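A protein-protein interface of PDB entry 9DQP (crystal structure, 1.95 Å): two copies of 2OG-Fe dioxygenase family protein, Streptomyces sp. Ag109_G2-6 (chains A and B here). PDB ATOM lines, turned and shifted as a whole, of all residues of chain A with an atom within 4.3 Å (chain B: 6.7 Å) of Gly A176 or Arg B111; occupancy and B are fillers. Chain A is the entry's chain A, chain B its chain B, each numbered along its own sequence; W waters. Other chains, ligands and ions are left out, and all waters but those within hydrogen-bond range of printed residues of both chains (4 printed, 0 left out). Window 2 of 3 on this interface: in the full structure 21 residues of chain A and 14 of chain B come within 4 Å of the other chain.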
ATOM      1  N   ARG A 171     -31.513  11.612  15.346  1.00  0.00           N
ATOM      2  CA  ARG A 171     -30.855  11.695  14.057  1.00  0.00           C
ATOM      3  C   ARG A 171     -30.955  13.156  13.662  1.00  0.00           C
ATOM      4  O   ARG A 171     -32.066  13.698  13.633  1.00  0.00           O
ATOM      5  CB  ARG A 171     -31.558  10.800  13.036  1.00  0.00           C
ATOM      6  CG  ARG A 171     -30.677  10.197  12.004  1.00  0.00           C
ATOM      7  CD  ARG A 171     -31.415   9.063  11.310  1.00  0.00           C
ATOM      8  NE  ARG A 171     -30.757   8.713  10.060  1.00  0.00           N
ATOM      9  CZ  ARG A 171     -31.092   9.235   8.888  1.00  0.00           C
ATOM     10  NH1 ARG A 171     -32.098  10.086   8.776  1.00  0.00           N
ATOM     11  NH2 ARG A 171     -30.397   8.898   7.805  1.00  0.00           N
ATOM     12  N   ALA A 175     -27.697  11.831   6.739  1.00  0.00           N
ATOM     13  CA  ALA A 175     -28.060  10.868   5.725  1.00  0.00           C
ATOM     14  C   ALA A 175     -27.112   9.685   5.856  1.00  0.00           C
ATOM     15  O   ALA A 175     -26.127   9.740   6.591  1.00  0.00           O
ATOM     16  CB  ALA A 175     -27.989  11.479   4.327  1.00  0.00           C
ATOM     17  N   GLY A 176     -27.405   8.608   5.134  1.00  0.00           N
ATOM     18  CA  GLY A 176     -26.622   7.408   5.328  1.00  0.00           C
ATOM     19  C   GLY A 176     -26.983   6.742   6.645  1.00  0.00           C
ATOM     20  O   GLY A 176     -28.087   6.892   7.167  1.00  0.00           O
ATOM     21  N   GLY A 177     -26.018   6.027   7.212  1.00  0.00           N
ATOM     22  CA  GLY A 177     -26.298   5.354   8.464  1.00  0.00           C
ATOM     23  C   GLY A 177     -27.206   4.152   8.327  1.00  0.00           C
ATOM     24  O   GLY A 177     -27.797   3.725   9.312  1.00  0.00           O
ATOM     25  N   GLU A 178     -27.363   3.618   7.118  1.00  0.00           N
ATOM     26  CA  GLU A 178     -28.188   2.428   6.936  1.00  0.00           C
ATOM     27  C   GLU A 178     -27.585   1.243   7.692  1.00  0.00           C
ATOM     28  O   GLU A 178     -26.365   1.059   7.713  1.00  0.00           O
ATOM     29  CB  GLU A 178     -28.311   2.092   5.443  1.00  0.00           C
ATOM     30  CG  GLU A 178     -28.969   3.190   4.606  1.00  0.00           C
ATOM     31  CD  GLU A 178     -27.971   4.197   4.052  1.00  0.00           C
ATOM     32  OE1 GLU A 178     -26.837   4.243   4.547  1.00  0.00           O
ATOM     33  OE2 GLU A 178     -28.317   4.948   3.114  1.00  0.00           O
ATOM     34  N   ARG A 213     -23.571   1.743   7.929  1.00  0.00           N
ATOM     35  CA  ARG A 213     -22.894   2.617   6.991  1.00  0.00           C
ATOM     36  C   ARG A 213     -22.551   3.941   7.662  1.00  0.00           C
ATOM     37  O   ARG A 213     -23.254   4.377   8.582  1.00  0.00           O
ATOM     38  CB  ARG A 213     -23.770   2.895   5.772  1.00  0.00           C
ATOM     39  CG  ARG A 213     -23.944   1.736   4.827  1.00  0.00           C
ATOM     40  CD  ARG A 213     -24.350   2.253   3.449  1.00  0.00           C
ATOM     41  NE  ARG A 213     -24.715   1.175   2.538  1.00  0.00           N
ATOM     42  CZ  ARG A 213     -23.850   0.551   1.748  1.00  0.00           C
ATOM     43  NH1 ARG A 213     -22.568   0.888   1.723  1.00  0.00           N
ATOM     44  NH2 ARG A 213     -24.279  -0.441   0.973  1.00  0.00           N
ATOM     45  N   PRO A 214     -21.491   4.609   7.204  1.00  0.00           N
ATOM     46  CA  PRO A 214     -21.196   5.960   7.706  1.00  0.00           C
ATOM     47  C   PRO A 214     -22.387   6.886   7.521  1.00  0.00           C
ATOM     48  O   PRO A 214     -23.237   6.669   6.656  1.00  0.00           O
ATOM     49  CB  PRO A 214     -20.011   6.409   6.842  1.00  0.00           C
ATOM     50  CG  PRO A 214     -19.410   5.135   6.315  1.00  0.00           C
ATOM     51  CD  PRO A 214     -20.558   4.183   6.149  1.00  0.00           C
ATOM     52  N   HIS A 216     -23.517  10.949   6.761  1.00  0.00           N
ATOM     53  CA  HIS A 216     -22.944  12.165   6.202  1.00  0.00           C
ATOM     54  C   HIS A 216     -23.983  13.245   6.286  1.00  0.00           C
ATOM     55  O   HIS A 216     -25.200  12.952   6.316  1.00  0.00           O
ATOM     56  CB  HIS A 216     -22.452  11.966   4.756  1.00  0.00           C
ATOM     57  CG  HIS A 216     -23.476  11.376   3.841  1.00  0.00           C
ATOM     58  ND1 HIS A 216     -23.465  10.047   3.477  1.00  0.00           N
ATOM     59  CD2 HIS A 216     -24.538  11.930   3.207  1.00  0.00           C
ATOM     60  CE1 HIS A 216     -24.476   9.805   2.664  1.00  0.00           C
ATOM     61  NE2 HIS A 216     -25.143  10.932   2.483  1.00  0.00           N
ATOM     62  N   GLU B  27     -20.029  12.765  -2.997  1.00  0.00           N
ATOM     63  CA  GLU B  27     -20.245  11.347  -2.728  1.00  0.00           C
ATOM     64  C   GLU B  27     -21.301  10.772  -3.669  1.00  0.00           C
ATOM     65  O   GLU B  27     -21.116   9.694  -4.246  1.00  0.00           O
ATOM     66  CB  GLU B  27     -20.649  11.150  -1.268  1.00  0.00           C
ATOM     67  CG  GLU B  27     -20.771   9.695  -0.844  1.00  0.00           C
ATOM     68  CD  GLU B  27     -21.622   9.529   0.403  1.00  0.00           C
ATOM     69  OE1 GLU B  27     -21.988  10.565   1.006  1.00  0.00           O
ATOM     70  OE2 GLU B  27     -21.935   8.371   0.775  1.00  0.00           O
ATOM     71  N   HIS B  31     -20.649   7.996  -6.601  1.00  0.00           N
ATOM     72  CA  HIS B  31     -21.344   6.716  -6.706  1.00  0.00           C
ATOM     73  C   HIS B  31     -22.150   6.606  -7.990  1.00  0.00           C
ATOM     74  O   HIS B  31     -22.352   5.494  -8.487  1.00  0.00           O
ATOM     75  CB  HIS B  31     -22.246   6.486  -5.496  1.00  0.00           C
ATOM     76  CG  HIS B  31     -21.491   6.226  -4.235  1.00  0.00           C
ATOM     77  ND1 HIS B  31     -20.617   5.167  -4.096  1.00  0.00           N
ATOM     78  CD2 HIS B  31     -21.471   6.891  -3.058  1.00  0.00           C
ATOM     79  CE1 HIS B  31     -20.100   5.188  -2.881  1.00  0.00           C
ATOM     80  NE2 HIS B  31     -20.604   6.222  -2.230  1.00  0.00           N
ATOM     81  N   ASN B 106     -22.860  -1.059  -4.430  1.00  0.00           N
ATOM     82  CA  ASN B 106     -22.927   0.405  -4.493  1.00  0.00           C
ATOM     83  C   ASN B 106     -24.071   0.925  -3.630  1.00  0.00           C
ATOM     84  O   ASN B 106     -25.236   0.601  -3.900  1.00  0.00           O
ATOM     85  CB  ASN B 106     -23.103   0.818  -5.952  1.00  0.00           C
ATOM     86  CG  ASN B 106     -22.935   2.304  -6.171  1.00  0.00           C
ATOM     87  OD1 ASN B 106     -23.290   3.122  -5.319  1.00  0.00           O
ATOM     88  ND2 ASN B 106     -22.412   2.661  -7.332  1.00  0.00           N
ATOM     89  N   PRO B 107     -23.811   1.746  -2.608  1.00  0.00           N
ATOM     90  CA  PRO B 107     -24.907   2.231  -1.756  1.00  0.00           C
ATOM     91  C   PRO B 107     -25.965   3.019  -2.493  1.00  0.00           C
ATOM     92  O   PRO B 107     -27.081   3.154  -1.974  1.00  0.00           O
ATOM     93  CB  PRO B 107     -24.198   3.125  -0.735  1.00  0.00           C
ATOM     94  CG  PRO B 107     -22.931   3.519  -1.413  1.00  0.00           C
ATOM     95  CD  PRO B 107     -22.512   2.306  -2.189  1.00  0.00           C
ATOM     96  N   LEU B 108     -25.646   3.557  -3.671  1.00  0.00           N
ATOM     97  CA  LEU B 108     -26.594   4.397  -4.385  1.00  0.00           C
ATOM     98  C   LEU B 108     -27.822   3.616  -4.827  1.00  0.00           C
ATOM     99  O   LEU B 108     -28.913   4.175  -4.910  1.00  0.00           O
ATOM    100  CB  LEU B 108     -25.904   5.036  -5.600  1.00  0.00           C
ATOM    101  CG  LEU B 108     -26.815   5.896  -6.473  1.00  0.00           C
ATOM    102  CD1 LEU B 108     -27.454   6.985  -5.638  1.00  0.00           C
ATOM    103  CD2 LEU B 108     -26.039   6.482  -7.641  1.00  0.00           C
ATOM    104  N   LEU B 109     -27.686   2.325  -5.100  1.00  0.00           N
ATOM    105  CA  LEU B 109     -28.827   1.596  -5.655  1.00  0.00           C
ATOM    106  C   LEU B 109     -30.002   1.564  -4.681  1.00  0.00           C
ATOM    107  O   LEU B 109     -31.135   1.915  -5.034  1.00  0.00           O
ATOM    108  CB  LEU B 109     -28.410   0.177  -6.029  1.00  0.00           C
ATOM    109  CG  LEU B 109     -29.469  -0.624  -6.790  1.00  0.00           C
ATOM    110  CD1 LEU B 109     -29.562  -0.210  -8.261  1.00  0.00           C
ATOM    111  CD2 LEU B 109     -29.179  -2.118  -6.653  1.00  0.00           C
ATOM    112  N   THR B 110     -29.763   1.108  -3.450  1.00  0.00           N
ATOM    113  CA  THR B 110     -30.872   1.058  -2.502  1.00  0.00           C
ATOM    114  C   THR B 110     -31.243   2.445  -2.001  1.00  0.00           C
ATOM    115  O   THR B 110     -32.390   2.649  -1.595  1.00  0.00           O
ATOM    116  CB  THR B 110     -30.574   0.148  -1.298  1.00  0.00           C
ATOM    117  OG1 THR B 110     -29.416   0.618  -0.587  1.00  0.00           O
ATOM    118  CG2 THR B 110     -30.370  -1.301  -1.743  1.00  0.00           C
ATOM    119  N   ARG B 111     -30.325   3.412  -2.049  1.00  0.00           N
ATOM    120  CA  ARG B 111     -30.719   4.773  -1.681  1.00  0.00           C
ATOM    121  C   ARG B 111     -31.685   5.359  -2.690  1.00  0.00           C
ATOM    122  O   ARG B 111     -32.632   6.052  -2.310  1.00  0.00           O
ATOM    123  CB  ARG B 111     -29.497   5.676  -1.535  1.00  0.00           C
ATOM    124  CG  ARG B 111     -28.676   5.296  -0.311  1.00  0.00           C
ATOM    125  CD  ARG B 111     -27.392   6.080  -0.194  1.00  0.00           C
ATOM    126  NE  ARG B 111     -26.824   5.925   1.141  1.00  0.00           N
ATOM    127  CZ  ARG B 111     -25.570   6.219   1.460  1.00  0.00           C
ATOM    128  NH1 ARG B 111     -24.718   6.672   0.552  1.00  0.00           N
ATOM    129  NH2 ARG B 111     -25.154   6.027   2.710  1.00  0.00           N
ATOM    130  N   LEU B 112     -31.444   5.122  -3.986  1.00  0.00           N
ATOM    131  CA  LEU B 112     -32.433   5.497  -4.993  1.00  0.00           C
ATOM    132  C   LEU B 112     -33.731   4.717  -4.811  1.00  0.00           C
ATOM    133  O   LEU B 112     -34.826   5.278  -4.936  1.00  0.00           O
ATOM    134  CB  LEU B 112     -31.882   5.241  -6.394  1.00  0.00           C
ATOM    135  CG  LEU B 112     -30.832   6.194  -6.939  1.00  0.00           C
ATOM    136  CD1 LEU B 112     -30.295   5.636  -8.271  1.00  0.00           C
ATOM    137  CD2 LEU B 112     -31.457   7.576  -7.091  1.00  0.00           C
ATOM    138  N   LEU B 113     -33.629   3.411  -4.562  1.00  0.00           N
ATOM    139  CA  LEU B 113     -34.834   2.627  -4.319  1.00  0.00           C
ATOM    140  C   LEU B 113     -35.705   3.295  -3.257  1.00  0.00           C
ATOM    141  O   LEU B 113     -36.900   3.496  -3.471  1.00  0.00           O
ATOM    142  CB  LEU B 113     -34.465   1.187  -3.929  1.00  0.00           C
ATOM    143  CG  LEU B 113     -35.635   0.186  -3.803  1.00  0.00           C
ATOM    144  CD1 LEU B 113     -35.192  -1.246  -4.075  1.00  0.00           C
ATOM    145  CD2 LEU B 113     -36.321   0.242  -2.416  1.00  0.00           C
ATOM    146  N   ARG B 114     -35.121   3.668  -2.104  1.00  0.00           N
ATOM    147  CA  ARG B 114     -35.936   4.261  -1.038  1.00  0.00           C
ATOM    148  C   ARG B 114     -36.368   5.676  -1.398  1.00  0.00           C
ATOM    149  O   ARG B 114     -37.524   6.065  -1.188  1.00  0.00           O
ATOM    150  CB  ARG B 114     -35.164   4.273   0.290  1.00  0.00           C
ATOM    151  CG  ARG B 114     -34.761   2.868   0.794  1.00  0.00           C
ATOM    152  CD  ARG B 114     -34.166   2.938   2.220  1.00  0.00           C
ATOM    153  NE  ARG B 114     -33.653   1.631   2.628  1.00  0.00           N
ATOM    154  CZ  ARG B 114     -32.406   1.232   2.430  1.00  0.00           C
ATOM    155  NH1 ARG B 114     -31.500   2.039   1.893  1.00  0.00           N
ATOM    156  NH2 ARG B 114     -32.073  -0.021   2.733  1.00  0.00           N
ATOM    157  N   ALA B 115     -35.447   6.478  -1.919  1.00  0.00           N
ATOM    158  CA  ALA B 115     -35.806   7.863  -2.219  1.00  0.00           C
ATOM    159  C   ALA B 115     -36.865   7.946  -3.310  1.00  0.00           C
ATOM    160  O   ALA B 115     -37.805   8.751  -3.217  1.00  0.00           O
ATOM    161  CB  ALA B 115     -34.558   8.653  -2.612  1.00  0.00           C
ATOM    162  N   ASP B 116     -36.731   7.141  -4.367  1.00  0.00           N
ATOM    163  CA  ASP B 116     -37.714   7.225  -5.445  1.00  0.00           C
ATOM    164  C   ASP B 116     -39.108   6.947  -4.916  1.00  0.00           C
ATOM    165  O   ASP B 116     -40.064   7.649  -5.258  1.00  0.00           O
ATOM    166  CB  ASP B 116     -37.376   6.244  -6.579  1.00  0.00           C
ATOM    167  CG  ASP B 116     -36.089   6.588  -7.295  1.00  0.00           C
ATOM    168  OD1 ASP B 116     -35.664   7.770  -7.267  1.00  0.00           O
ATOM    169  OD2 ASP B 116     -35.491   5.674  -7.897  1.00  0.00           O
HETATM  170  O   HOH W   1     -31.251   4.915   1.799  1.00  0.00           O
HETATM  171  O   HOH W   2     -27.212   1.717   0.801  1.00  0.00           O
HETATM  172  O   HOH W   3     -22.663   6.698   4.007  1.00  0.00           O
HETATM  173  O   HOH W   4     -26.706  -1.041  -0.184  1.00  0.00           O
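The guanidinium group (NE) of Arg B111 is in salt-bridge range of the side-chain carboxylate (OE2) of Glu A178 (2.7 Å).
A ring nitrogen (ND1) of His A216 lies within hydrogen-bond range of the side-chain carboxylate of Glu B27.
NH2 of Arg A171 lies within hydrogen-bond range of O of Gly A176 (3.1 Å).
The backbone carbonyl oxygen (O) of His A216 sits at hydrogen-bond distance from the backbone NH (N) of Ala A175, 2.8 Å away.
O of Arg A213 lies close to N of Gly A177, at 3.5 Å.
The backbone carbonyl oxygen of Glu A178 lies within hydrogen-bond range of the backbone NH of Arg A213, at 2.9 Å.
The guanidinium group (NH1) of Arg B111 lies within salt-bridge range of the side-chain carboxylate (OE2) of Glu B27 (3.3 Å).
Arg B111 touches Gly A176 (NH2 to CA, 3.3 Å).
Glu A178 touches Arg B114.
Arg A213 touches Pro B107.
Arg B111 touches Arg A213.
Arg B111 touches His A216 (NH1 to CE1, 3.8 Å).
Gly A176 touches just one residue of chain B: Arg B111.
Of the printed residues of chain B, Glu A178 touches Arg B111 (2.7 Å) and Arg B114 (3.9 Å).
Of the printed residues of chain B, His A216 touches Glu B27 and Arg B111.
Of the printed residues of chain A, Glu B27 touches His A216 (2.9 Å).
Of the printed residues of chain A, Pro B107 touches Arg A213.
Leu B109 touches none of the printed residues of chain A.
Leu B113 touches none of the printed residues of chain A.
Printed residues of chain A within 4 Å of Arg B114: Glu A178.
The nearest printed residue of chain A that does not touch Arg B111 is Pro A214 (4.4 Å).
The nearest printed residue of chain A that does not touch Glu B27 is Pro A214 (6.3 Å).
Of the 8 printed residues of chain A, 4 touch a printed residue of chain B.
Hydrophobic or aromatic side chains of chain A within 4 Å of the printed part of chain B: His A216.
Along chain A the printed residues that touch a printed residue of chain B span positions 176 to 216.
Printed residues of chain B that touch a printed residue of chain A: Glu B27, Pro B107, Arg B111 and Arg B114.
Hydrophobic or aromatic side chains of chain B within 4 Å of the printed part of chain A: Pro B107.
Among the printed residues, Asp or Glu carboxylates within 4 Å of a Lys or Arg side-chain nitrogen of the other chain: Glu A178 with Arg B111.
No position is printed for both chains.
Water W3 lies within hydrogen-bond range of the backbone carbonyl oxygen (O) of Pro A214 (2.7 Å), the guanidinium group (NH2) of Arg B111 (2.9 Å) and a ring nitrogen (ND1) of His A216 (3.5 Å).
Water W4 bridges NH2 of Arg A213 (2.8 Å) and OG1 of Thr B110 (3.2 Å).
Water W2 lies within hydrogen-bond range of the side-chain hydroxyl of Thr B110 (2.8 Å), the guanidinium group of Arg A213 (3.1 Å) and the backbone carbonyl oxygen of Pro B107 (3.1 Å).
Water W1 bridges the guanidinium group (NH1) of Arg B114 and the side-chain carboxylate (OE2) of Glu A178.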
